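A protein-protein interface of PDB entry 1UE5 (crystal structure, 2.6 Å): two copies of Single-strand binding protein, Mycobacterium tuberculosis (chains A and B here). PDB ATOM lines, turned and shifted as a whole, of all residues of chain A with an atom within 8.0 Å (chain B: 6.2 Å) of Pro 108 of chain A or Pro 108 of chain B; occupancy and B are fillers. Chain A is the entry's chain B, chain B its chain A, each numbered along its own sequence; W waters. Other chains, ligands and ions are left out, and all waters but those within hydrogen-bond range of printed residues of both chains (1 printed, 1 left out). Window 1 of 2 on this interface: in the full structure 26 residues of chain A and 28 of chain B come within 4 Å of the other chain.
The guanidinium group (NH2) of Arg 76 of chain B is in salt-bridge range of the side-chain carboxylate (OE2) of Glu 105 of chain A, 2.4 Å away.
The backbone NH of Leu 110 of chain A is in hydrogen-bond range of the backbone carbonyl oxygen of Ile 106 of chain B, at 3.0 Å.
OE1 of Glu 105 of chain A is in hydrogen-bond range of OG of Ser 109 of chain B, 2.5 Å away.
N of Leu 110 of chain B is in hydrogen-bond range of O of Ile 106 of chain A (2.8 Å).
The backbone NH (N) of Ala 115 of chain B sits at hydrogen-bond distance from the side-chain hydroxyl (OG) of Ser 70 of chain A.
O of Ala 115 of chain A lies close to O of Ser 70 of chain B (3.2 Å).
The backbone carbonyl oxygen (O) of Arg 76 of chain B sits at hydrogen-bond distance from the backbone NH (N) of Ser 109 of chain B.
The backbone carbonyl oxygen (O) of Gly 107 of chain B lies within hydrogen-bond range of the backbone NH (N) of Ile 78 of chain B, 2.8 Å away.
The backbone carbonyl oxygen (O) of Arg 76 of chain A is in hydrogen-bond range of the backbone NH (N) of Ser 109 of chain A, at 2.8 Å.
The backbone NH of Ile 78 of chain A sits at hydrogen-bond distance from the backbone carbonyl oxygen of Gly 107 of chain A (3.1 Å).
The side-chain hydroxyl (OG) of Ser 109 of chain A lies close to the backbone NH (N) of Arg 111 of chain A (3.2 Å).
CG of Leu 71 of chain A touches CD1 of Leu 110 of chain B, 3.8 Å away.
Glu 105 of chain A touches Ile 78 of chain B.
Ile 78 of chain B touches Ile 106 of chain A (CD1 to N, 3.1 Å).
O of Ile 106 of chain A touches CA of Ser 109 of chain B (3.7 Å).
Ile 78 of chain B touches Gly 107 of chain A (CD1 to N, 3.6 Å).
CA of Gly 107 of chain A touches O of Pro 108 of chain B (3.0 Å).
Pro 108 of chain A touches Gly 107 of chain B (O to CA, 3.2 Å).
CB of Pro 108 of chain A touches CG2 of Val 117 of chain B (3.3 Å).
Ser 109 of chain A touches Ile 106 of chain B (CA to O, 3.8 Å).
Thr 114 of chain A touches Val 117 of chain B (O to CA, 3.8 Å).
Of the printed residues of chain B, Pro 108 of chain A touches Gly 107 (3.2 Å), Pro 108 (3.5 Å) and Val 117 (3.3 Å).
Of chain A, only Gly 107 (3.0 Å), Pro 108 (3.5 Å) and Val 117 (3.3 Å) come within 4 Å of Pro 108 of chain B.
Of the printed residues of chain A, Ile 78 of chain B touches Ile 78, Glu 105, Ile 106 and Gly 107.
Printed residues of chain B within 4 Å of Ile 78 of chain A: Ile 78.
Of the printed residues of chain A, Ser 109 of chain B touches Glu 105 and Ile 106.
Of the printed residues of chain A, Val 117 of chain B touches Pro 108 and Thr 114.
Printed residues of chain B within 4 Å of Lys 116 of chain A: Ala 115 (3.2 Å).
Hydrophobic or aromatic side chains of chain A within 4 Å of the printed part of chain B: Leu 71, Ile 78, Pro 108, Leu 110 and Val 117.
Along chain A the printed residues that touch a printed residue of chain B span positions 70 to 117.
Of the 13 printed residues of chain B, 11 touch a printed residue of chain A.
Among the printed residues, 25 pairs touch across the chains.
Among the printed residues, Asp or Glu carboxylates within 4 Å of a Lys or Arg side-chain nitrogen of the other chain: Glu 105 of chain A with Arg 76 of chain B (2.4 Å).
Ile 106 of chain A touches Ile 78 of chain B, but with the chains exchanged Ile 78 of chain A does not touch Ile 106 of chain B (4.6 Å).
Gly 107 of chain A touches Ile 78 of chain B, but with the chains exchanged Ile 78 of chain A does not touch Gly 107 of chain B (4.3 Å).
Gly 107 of chain A touches Pro 108 of chain B, and with the chains exchanged Pro 108 of chain A touches Gly 107 of chain B.
Val 117 of chain A touches Ala 115 of chain B, but with the chains exchanged Ala 115 of chain A does not touch Val 117 of chain B (4.3 Å).
Water W1 lies within hydrogen-bond range of the backbone NH of Val 117 of chain B and the backbone carbonyl oxygen of Ser 70 of chain A.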
ATOM      1  N   GLY A  11      -7.504 -27.908 -18.028  1.00  0.00           N
ATOM      2  CA  GLY A  11      -6.428 -28.808 -18.398  1.00  0.00           C
ATOM      3  C   GLY A  11      -5.369 -28.100 -19.213  1.00  0.00           C
ATOM      4  O   GLY A  11      -5.439 -26.884 -19.399  1.00  0.00           O
ATOM      5  N   SER A  70      -2.242 -16.637 -28.656  1.00  0.00           N
ATOM      6  CA  SER A  70      -1.952 -16.610 -27.224  1.00  0.00           C
ATOM      7  C   SER A  70      -1.519 -17.935 -26.604  1.00  0.00           C
ATOM      8  O   SER A  70      -0.647 -17.958 -25.742  1.00  0.00           O
ATOM      9  CB  SER A  70      -3.184 -16.105 -26.476  1.00  0.00           C
ATOM     10  OG  SER A  70      -3.812 -15.049 -27.179  1.00  0.00           O
ATOM     11  N   LEU A  71      -2.131 -19.033 -27.031  1.00  0.00           N
ATOM     12  CA  LEU A  71      -1.819 -20.337 -26.464  1.00  0.00           C
ATOM     13  C   LEU A  71      -0.802 -21.186 -27.210  1.00  0.00           C
ATOM     14  O   LEU A  71      -0.740 -21.196 -28.441  1.00  0.00           O
ATOM     15  CB  LEU A  71      -3.104 -21.152 -26.296  1.00  0.00           C
ATOM     16  CG  LEU A  71      -4.290 -20.450 -25.639  1.00  0.00           C
ATOM     17  CD1 LEU A  71      -5.394 -21.462 -25.375  1.00  0.00           C
ATOM     18  CD2 LEU A  71      -3.843 -19.795 -24.348  1.00  0.00           C
ATOM     19  N   ALA A  75       0.030 -25.148 -22.106  1.00  0.00           N
ATOM     20  CA  ALA A  75      -0.586 -24.050 -21.389  1.00  0.00           C
ATOM     21  C   ALA A  75      -1.803 -24.594 -20.660  1.00  0.00           C
ATOM     22  O   ALA A  75      -2.479 -25.497 -21.153  1.00  0.00           O
ATOM     23  CB  ALA A  75      -0.989 -22.940 -22.359  1.00  0.00           C
ATOM     24  N   ARG A  76      -2.066 -24.058 -19.474  1.00  0.00           N
ATOM     25  CA  ARG A  76      -3.212 -24.487 -18.683  1.00  0.00           C
ATOM     26  C   ARG A  76      -4.374 -23.612 -19.105  1.00  0.00           C
ATOM     27  O   ARG A  76      -4.278 -22.382 -19.078  1.00  0.00           O
ATOM     28  CB  ARG A  76      -2.944 -24.288 -17.191  1.00  0.00           C
ATOM     29  CG  ARG A  76      -4.017 -24.879 -16.316  1.00  0.00           C
ATOM     30  CD  ARG A  76      -3.798 -24.561 -14.850  1.00  0.00           C
ATOM     31  NE  ARG A  76      -4.805 -25.247 -14.049  1.00  0.00           N
ATOM     32  CZ  ARG A  76      -4.770 -26.546 -13.769  1.00  0.00           C
ATOM     33  NH1 ARG A  76      -3.766 -27.295 -14.207  1.00  0.00           N
ATOM     34  NH2 ARG A  76      -5.761 -27.106 -13.096  1.00  0.00           N
ATOM     35  N   VAL A  77      -5.479 -24.238 -19.480  1.00  0.00           N
ATOM     36  CA  VAL A  77      -6.629 -23.477 -19.926  1.00  0.00           C
ATOM     37  C   VAL A  77      -7.958 -23.953 -19.337  1.00  0.00           C
ATOM     38  O   VAL A  77      -8.091 -25.104 -18.924  1.00  0.00           O
ATOM     39  CB  VAL A  77      -6.722 -23.538 -21.467  1.00  0.00           C
ATOM     40  CG1 VAL A  77      -5.421 -23.092 -22.074  1.00  0.00           C
ATOM     41  CG2 VAL A  77      -7.033 -24.954 -21.915  1.00  0.00           C
ATOM     42  N   ILE A  78      -8.932 -23.051 -19.292  1.00  0.00           N
ATOM     43  CA  ILE A  78     -10.268 -23.387 -18.821  1.00  0.00           C
ATOM     44  C   ILE A  78     -11.179 -23.180 -20.037  1.00  0.00           C
ATOM     45  O   ILE A  78     -11.217 -22.106 -20.634  1.00  0.00           O
ATOM     46  CB  ILE A  78     -10.690 -22.499 -17.614  1.00  0.00           C
ATOM     47  CG1 ILE A  78     -12.215 -22.465 -17.495  1.00  0.00           C
ATOM     48  CG2 ILE A  78     -10.057 -21.133 -17.728  1.00  0.00           C
ATOM     49  CD1 ILE A  78     -12.714 -21.623 -16.346  1.00  0.00           C
ATOM     50  N   VAL A  79     -11.902 -24.225 -20.405  1.00  0.00           N
ATOM     51  CA  VAL A  79     -12.751 -24.192 -21.586  1.00  0.00           C
ATOM     52  C   VAL A  79     -14.236 -24.401 -21.320  1.00  0.00           C
ATOM     53  O   VAL A  79     -14.628 -25.277 -20.550  1.00  0.00           O
ATOM     54  CB  VAL A  79     -12.279 -25.285 -22.590  1.00  0.00           C
ATOM     55  CG1 VAL A  79     -13.167 -25.322 -23.820  1.00  0.00           C
ATOM     56  CG2 VAL A  79     -10.839 -25.033 -22.978  1.00  0.00           C
ATOM     57  N   GLU A 105     -16.023 -20.366 -25.235  1.00  0.00           N
ATOM     58  CA  GLU A 105     -15.104 -19.451 -24.577  1.00  0.00           C
ATOM     59  C   GLU A 105     -13.913 -20.243 -24.044  1.00  0.00           C
ATOM     60  O   GLU A 105     -14.045 -21.405 -23.644  1.00  0.00           O
ATOM     61  CB  GLU A 105     -15.802 -18.749 -23.412  1.00  0.00           C
ATOM     62  CG  GLU A 105     -17.004 -17.922 -23.803  1.00  0.00           C
ATOM     63  CD  GLU A 105     -16.712 -16.448 -23.800  1.00  0.00           C
ATOM     64  OE1 GLU A 105     -15.523 -16.077 -23.880  1.00  0.00           O
ATOM     65  OE2 GLU A 105     -17.676 -15.660 -23.724  1.00  0.00           O
ATOM     66  N   ILE A 106     -12.747 -19.607 -24.050  1.00  0.00           N
ATOM     67  CA  ILE A 106     -11.536 -20.232 -23.551  1.00  0.00           C
ATOM     68  C   ILE A 106     -10.536 -19.148 -23.196  1.00  0.00           C
ATOM     69  O   ILE A 106     -10.522 -18.071 -23.802  1.00  0.00           O
ATOM     70  CB  ILE A 106     -10.899 -21.184 -24.588  1.00  0.00           C
ATOM     71  CG1 ILE A 106      -9.677 -21.870 -23.956  1.00  0.00           C
ATOM     72  CG2 ILE A 106     -10.523 -20.408 -25.851  1.00  0.00           C
ATOM     73  CD1 ILE A 106      -8.940 -22.865 -24.847  1.00  0.00           C
ATOM     74  N   GLY A 107      -9.714 -19.440 -22.193  1.00  0.00           N
ATOM     75  CA  GLY A 107      -8.707 -18.500 -21.744  1.00  0.00           C
ATOM     76  C   GLY A 107      -7.676 -19.218 -20.904  1.00  0.00           C
ATOM     77  O   GLY A 107      -7.919 -20.322 -20.418  1.00  0.00           O
ATOM     78  N   PRO A 108      -6.494 -18.625 -20.732  1.00  0.00           N
ATOM     79  CA  PRO A 108      -5.447 -19.258 -19.924  1.00  0.00           C
ATOM     80  C   PRO A 108      -5.732 -19.201 -18.426  1.00  0.00           C
ATOM     81  O   PRO A 108      -6.023 -18.136 -17.890  1.00  0.00           O
ATOM     82  CB  PRO A 108      -4.205 -18.455 -20.287  1.00  0.00           C
ATOM     83  CG  PRO A 108      -4.772 -17.078 -20.591  1.00  0.00           C
ATOM     84  CD  PRO A 108      -5.984 -17.426 -21.421  1.00  0.00           C
ATOM     85  N   SER A 109      -5.642 -20.346 -17.757  1.00  0.00           N
ATOM     86  CA  SER A 109      -5.875 -20.399 -16.315  1.00  0.00           C
ATOM     87  C   SER A 109      -4.803 -19.624 -15.578  1.00  0.00           C
ATOM     88  O   SER A 109      -3.618 -19.823 -15.822  1.00  0.00           O
ATOM     89  CB  SER A 109      -5.848 -21.834 -15.802  1.00  0.00           C
ATOM     90  OG  SER A 109      -5.926 -21.825 -14.391  1.00  0.00           O
ATOM     91  N   LEU A 110      -5.218 -18.750 -14.670  1.00  0.00           N
ATOM     92  CA  LEU A 110      -4.276 -17.956 -13.893  1.00  0.00           C
ATOM     93  C   LEU A 110      -3.914 -18.649 -12.584  1.00  0.00           C
ATOM     94  O   LEU A 110      -3.536 -17.993 -11.611  1.00  0.00           O
ATOM     95  CB  LEU A 110      -4.867 -16.585 -13.577  1.00  0.00           C
ATOM     96  CG  LEU A 110      -5.170 -15.677 -14.757  1.00  0.00           C
ATOM     97  CD1 LEU A 110      -5.685 -14.352 -14.231  1.00  0.00           C
ATOM     98  CD2 LEU A 110      -3.915 -15.469 -15.586  1.00  0.00           C
ATOM     99  N   ARG A 111      -4.031 -19.973 -12.560  1.00  0.00           N
ATOM    100  CA  ARG A 111      -3.719 -20.739 -11.362  1.00  0.00           C
ATOM    101  C   ARG A 111      -2.242 -20.684 -11.042  1.00  0.00           C
ATOM    102  O   ARG A 111      -1.857 -20.390  -9.913  1.00  0.00           O
ATOM    103  CB  ARG A 111      -4.141 -22.188 -11.537  1.00  0.00           C
ATOM    104  CG  ARG A 111      -4.025 -23.014 -10.279  1.00  0.00           C
ATOM    105  CD  ARG A 111      -5.055 -24.118 -10.330  1.00  0.00           C
ATOM    106  NE  ARG A 111      -5.292 -24.741  -9.037  1.00  0.00           N
ATOM    107  CZ  ARG A 111      -6.411 -25.385  -8.738  1.00  0.00           C
ATOM    108  NH1 ARG A 111      -7.379 -25.473  -9.641  1.00  0.00           N
ATOM    109  NH2 ARG A 111      -6.567 -25.940  -7.543  1.00  0.00           N
ATOM    110  N   TYR A 112      -1.410 -20.981 -12.034  1.00  0.00           N
ATOM    111  CA  TYR A 112       0.030 -20.949 -11.831  1.00  0.00           C
ATOM    112  C   TYR A 112       0.683 -19.954 -12.773  1.00  0.00           C
ATOM    113  O   TYR A 112       1.873 -20.063 -13.059  1.00  0.00           O
ATOM    114  CB  TYR A 112       0.656 -22.324 -12.082  1.00  0.00           C
ATOM    115  CG  TYR A 112      -0.041 -23.484 -11.417  1.00  0.00           C
ATOM    116  CD1 TYR A 112      -0.824 -24.365 -12.163  1.00  0.00           C
ATOM    117  CD2 TYR A 112       0.098 -23.721 -10.049  1.00  0.00           C
ATOM    118  CE1 TYR A 112      -1.450 -25.452 -11.566  1.00  0.00           C
ATOM    119  CE2 TYR A 112      -0.528 -24.809  -9.439  1.00  0.00           C
ATOM    120  CZ  TYR A 112      -1.296 -25.671 -10.208  1.00  0.00           C
ATOM    121  OH  TYR A 112      -1.902 -26.760  -9.631  1.00  0.00           O
ATOM    122  N   ALA A 113      -0.071 -18.979 -13.263  1.00  0.00           N
ATOM    123  CA  ALA A 113       0.525 -18.026 -14.189  1.00  0.00           C
ATOM    124  C   ALA A 113      -0.218 -16.712 -14.338  1.00  0.00           C
ATOM    125  O   ALA A 113      -1.427 -16.641 -14.146  1.00  0.00           O
ATOM    126  CB  ALA A 113       0.682 -18.678 -15.553  1.00  0.00           C
ATOM    127  N   THR A 114       0.527 -15.671 -14.686  1.00  0.00           N
ATOM    128  CA  THR A 114      -0.047 -14.356 -14.901  1.00  0.00           C
ATOM    129  C   THR A 114      -0.263 -14.169 -16.415  1.00  0.00           C
ATOM    130  O   THR A 114       0.017 -15.081 -17.203  1.00  0.00           O
ATOM    131  CB  THR A 114       0.887 -13.258 -14.347  1.00  0.00           C
ATOM    132  OG1 THR A 114       2.198 -13.406 -14.903  1.00  0.00           O
ATOM    133  CG2 THR A 114       0.984 -13.363 -12.844  1.00  0.00           C
ATOM    134  N   ALA A 115      -0.768 -13.004 -16.819  1.00  0.00           N
ATOM    135  CA  ALA A 115      -1.011 -12.732 -18.236  1.00  0.00           C
ATOM    136  C   ALA A 115      -1.373 -11.279 -18.514  1.00  0.00           C
ATOM    137  O   ALA A 115      -2.105 -10.653 -17.744  1.00  0.00           O
ATOM    138  CB  ALA A 115      -2.123 -13.639 -18.755  1.00  0.00           C
ATOM    139  N   LYS A 116      -0.850 -10.741 -19.612  1.00  0.00           N
ATOM    140  CA  LYS A 116      -1.165  -9.371 -19.991  1.00  0.00           C
ATOM    141  C   LYS A 116      -2.189  -9.434 -21.107  1.00  0.00           C
ATOM    142  O   LYS A 116      -1.839  -9.640 -22.267  1.00  0.00           O
ATOM    143  CB  LYS A 116       0.068  -8.621 -20.496  1.00  0.00           C
ATOM    144  CG  LYS A 116      -0.289  -7.232 -21.026  1.00  0.00           C
ATOM    145  CD  LYS A 116       0.912  -6.410 -21.466  1.00  0.00           C
ATOM    146  CE  LYS A 116       0.462  -5.024 -21.924  1.00  0.00           C
ATOM    147  NZ  LYS A 116       1.597  -4.102 -22.218  1.00  0.00           N
ATOM    148  N   VAL A 117      -3.456  -9.264 -20.758  1.00  0.00           N
ATOM    149  CA  VAL A 117      -4.507  -9.317 -21.758  1.00  0.00           C
ATOM    150  C   VAL A 117      -4.479  -8.071 -22.626  1.00  0.00           C
ATOM    151  O   VAL A 117      -3.987  -7.030 -22.205  1.00  0.00           O
ATOM    152  CB  VAL A 117      -5.885  -9.430 -21.102  1.00  0.00           C
ATOM    153  CG1 VAL A 117      -6.944  -9.654 -22.165  1.00  0.00           C
ATOM    154  CG2 VAL A 117      -5.881 -10.564 -20.094  1.00  0.00           C
ATOM    155  N   ASN A 118      -5.012  -8.186 -23.838  1.00  0.00           N
ATOM    156  CA  ASN A 118      -5.049  -7.069 -24.770  1.00  0.00           C
ATOM    157  C   ASN A 118      -6.326  -7.115 -25.609  1.00  0.00           C
ATOM    158  O   ASN A 118      -6.416  -7.890 -26.562  1.00  0.00           O
ATOM    159  CB  ASN A 118      -3.821  -7.124 -25.680  1.00  0.00           C
ATOM    160  CG  ASN A 118      -3.658  -5.872 -26.514  1.00  0.00           C
ATOM    161  OD1 ASN A 118      -2.718  -5.760 -27.301  1.00  0.00           O
ATOM    162  ND2 ASN A 118      -4.569  -4.919 -26.345  1.00  0.00           N
ATOM    163  N   SER B  70      -2.967  -9.415 -13.250  1.00  0.00           N
ATOM    164  CA  SER B  70      -3.197  -9.899 -14.597  1.00  0.00           C
ATOM    165  C   SER B  70      -4.510  -9.389 -15.191  1.00  0.00           C
ATOM    166  O   SER B  70      -4.649  -9.307 -16.409  1.00  0.00           O
ATOM    167  CB  SER B  70      -3.196 -11.426 -14.587  1.00  0.00           C
ATOM    168  OG  SER B  70      -2.140 -11.924 -13.780  1.00  0.00           O
ATOM    169  N   LEU B  71      -5.469  -9.043 -14.338  1.00  0.00           N
ATOM    170  CA  LEU B  71      -6.762  -8.564 -14.819  1.00  0.00           C
ATOM    171  C   LEU B  71      -7.087  -7.155 -14.324  1.00  0.00           C
ATOM    172  O   LEU B  71      -6.603  -6.726 -13.275  1.00  0.00           O
ATOM    173  CB  LEU B  71      -7.872  -9.529 -14.378  1.00  0.00           C
ATOM    174  CG  LEU B  71      -7.709 -11.003 -14.753  1.00  0.00           C
ATOM    175  CD1 LEU B  71      -8.766 -11.848 -14.050  1.00  0.00           C
ATOM    176  CD2 LEU B  71      -7.810 -11.151 -16.258  1.00  0.00           C
ATOM    177  N   ALA B  75     -12.161  -6.473 -17.972  1.00  0.00           N
ATOM    178  CA  ALA B  75     -11.678  -7.747 -18.472  1.00  0.00           C
ATOM    179  C   ALA B  75     -12.775  -8.805 -18.562  1.00  0.00           C
ATOM    180  O   ALA B  75     -13.532  -9.012 -17.608  1.00  0.00           O
ATOM    181  CB  ALA B  75     -10.549  -8.250 -17.590  1.00  0.00           C
ATOM    182  N   ARG B  76     -12.852  -9.458 -19.722  1.00  0.00           N
ATOM    183  CA  ARG B  76     -13.815 -10.528 -19.957  1.00  0.00           C
ATOM    184  C   ARG B  76     -13.152 -11.825 -19.473  1.00  0.00           C
ATOM    185  O   ARG B  76     -12.098 -12.222 -19.981  1.00  0.00           O
ATOM    186  CB  ARG B  76     -14.145 -10.649 -21.447  1.00  0.00           C
ATOM    187  CG  ARG B  76     -15.327 -11.560 -21.707  1.00  0.00           C
ATOM    188  CD  ARG B  76     -15.359 -12.101 -23.119  1.00  0.00           C
ATOM    189  NE  ARG B  76     -16.494 -13.004 -23.292  1.00  0.00           N
ATOM    190  CZ  ARG B  76     -17.768 -12.621 -23.231  1.00  0.00           C
ATOM    191  NH1 ARG B  76     -18.074 -11.349 -23.006  1.00  0.00           N
ATOM    192  NH2 ARG B  76     -18.739 -13.509 -23.394  1.00  0.00           N
ATOM    193  N   VAL B  77     -13.771 -12.492 -18.505  1.00  0.00           N
ATOM    194  CA  VAL B  77     -13.184 -13.706 -17.951  1.00  0.00           C
ATOM    195  C   VAL B  77     -14.104 -14.915 -17.855  1.00  0.00           C
ATOM    196  O   VAL B  77     -15.324 -14.781 -17.798  1.00  0.00           O
ATOM    197  CB  VAL B  77     -12.666 -13.442 -16.544  1.00  0.00           C
ATOM    198  CG1 VAL B  77     -11.671 -12.299 -16.554  1.00  0.00           C
ATOM    199  CG2 VAL B  77     -13.835 -13.118 -15.634  1.00  0.00           C
ATOM    200  N   ILE B  78     -13.491 -16.094 -17.820  1.00  0.00           N
ATOM    201  CA  ILE B  78     -14.213 -17.353 -17.676  1.00  0.00           C
ATOM    202  C   ILE B  78     -13.949 -17.825 -16.244  1.00  0.00           C
ATOM    203  O   ILE B  78     -12.811 -18.135 -15.885  1.00  0.00           O
ATOM    204  CB  ILE B  78     -13.694 -18.413 -18.648  1.00  0.00           C
ATOM    205  CG1 ILE B  78     -13.652 -17.832 -20.057  1.00  0.00           C
ATOM    206  CG2 ILE B  78     -14.595 -19.640 -18.604  1.00  0.00           C
ATOM    207  CD1 ILE B  78     -13.111 -18.777 -21.082  1.00  0.00           C
ATOM    208  N   ILE B 106      -9.862 -19.294 -12.876  1.00  0.00           N
ATOM    209  CA  ILE B 106     -10.282 -18.118 -13.602  1.00  0.00           C
ATOM    210  C   ILE B 106      -9.251 -17.763 -14.657  1.00  0.00           C
ATOM    211  O   ILE B 106      -8.049 -17.931 -14.442  1.00  0.00           O
ATOM    212  CB  ILE B 106     -10.469 -16.927 -12.639  1.00  0.00           C
ATOM    213  CG1 ILE B 106     -10.845 -15.676 -13.417  1.00  0.00           C
ATOM    214  CG2 ILE B 106      -9.187 -16.676 -11.867  1.00  0.00           C
ATOM    215  CD1 ILE B 106     -11.180 -14.506 -12.524  1.00  0.00           C
ATOM    216  N   GLY B 107      -9.731 -17.283 -15.799  1.00  0.00           N
ATOM    217  CA  GLY B 107      -8.837 -16.901 -16.873  1.00  0.00           C
ATOM    218  C   GLY B 107      -9.460 -15.842 -17.757  1.00  0.00           C
ATOM    219  O   GLY B 107     -10.685 -15.785 -17.878  1.00  0.00           O
ATOM    220  N   PRO B 108      -8.646 -14.968 -18.368  1.00  0.00           N
ATOM    221  CA  PRO B 108      -9.189 -13.926 -19.242  1.00  0.00           C
ATOM    222  C   PRO B 108      -9.636 -14.628 -20.512  1.00  0.00           C
ATOM    223  O   PRO B 108      -8.995 -15.587 -20.950  1.00  0.00           O
ATOM    224  CB  PRO B 108      -7.993 -13.014 -19.461  1.00  0.00           C
ATOM    225  CG  PRO B 108      -6.850 -13.984 -19.486  1.00  0.00           C
ATOM    226  CD  PRO B 108      -7.174 -14.903 -18.321  1.00  0.00           C
ATOM    227  N   SER B 109     -10.738 -14.174 -21.096  1.00  0.00           N
ATOM    228  CA  SER B 109     -11.248 -14.821 -22.299  1.00  0.00           C
ATOM    229  C   SER B 109     -10.543 -14.368 -23.554  1.00  0.00           C
ATOM    230  O   SER B 109     -10.256 -13.183 -23.726  1.00  0.00           O
ATOM    231  CB  SER B 109     -12.749 -14.576 -22.462  1.00  0.00           C
ATOM    232  OG  SER B 109     -13.231 -15.231 -23.625  1.00  0.00           O
ATOM    233  N   LEU B 110     -10.265 -15.327 -24.429  1.00  0.00           N
ATOM    234  CA  LEU B 110      -9.607 -15.039 -25.692  1.00  0.00           C
ATOM    235  C   LEU B 110     -10.657 -14.894 -26.784  1.00  0.00           C
ATOM    236  O   LEU B 110     -10.375 -15.102 -27.963  1.00  0.00           O
ATOM    237  CB  LEU B 110      -8.620 -16.156 -26.048  1.00  0.00           C
ATOM    238  CG  LEU B 110      -7.495 -16.370 -25.035  1.00  0.00           C
ATOM    239  CD1 LEU B 110      -6.539 -17.426 -25.556  1.00  0.00           C
ATOM    240  CD2 LEU B 110      -6.768 -15.055 -24.790  1.00  0.00           C
ATOM    241  N   ALA B 115      -3.453 -12.383 -25.296  1.00  0.00           N
ATOM    242  CA  ALA B 115      -2.702 -12.200 -24.063  1.00  0.00           C
ATOM    243  C   ALA B 115      -1.519 -13.145 -24.078  1.00  0.00           C
ATOM    244  O   ALA B 115      -1.659 -14.311 -24.443  1.00  0.00           O
ATOM    245  CB  ALA B 115      -3.586 -12.505 -22.865  1.00  0.00           C
ATOM    246  N   VAL B 117       0.734 -15.341 -22.105  1.00  0.00           N
ATOM    247  CA  VAL B 117       0.849 -16.022 -20.830  1.00  0.00           C
ATOM    248  C   VAL B 117       2.298 -16.219 -20.435  1.00  0.00           C
ATOM    249  O   VAL B 117       3.168 -16.379 -21.287  1.00  0.00           O
ATOM    250  CB  VAL B 117       0.180 -17.397 -20.904  1.00  0.00           C
ATOM    251  CG1 VAL B 117       0.318 -18.119 -19.586  1.00  0.00           C
ATOM    252  CG2 VAL B 117      -1.268 -17.233 -21.275  1.00  0.00           C
HETATM  253  O   HOH W   1       1.298 -16.214 -24.447  1.00  0.00           O
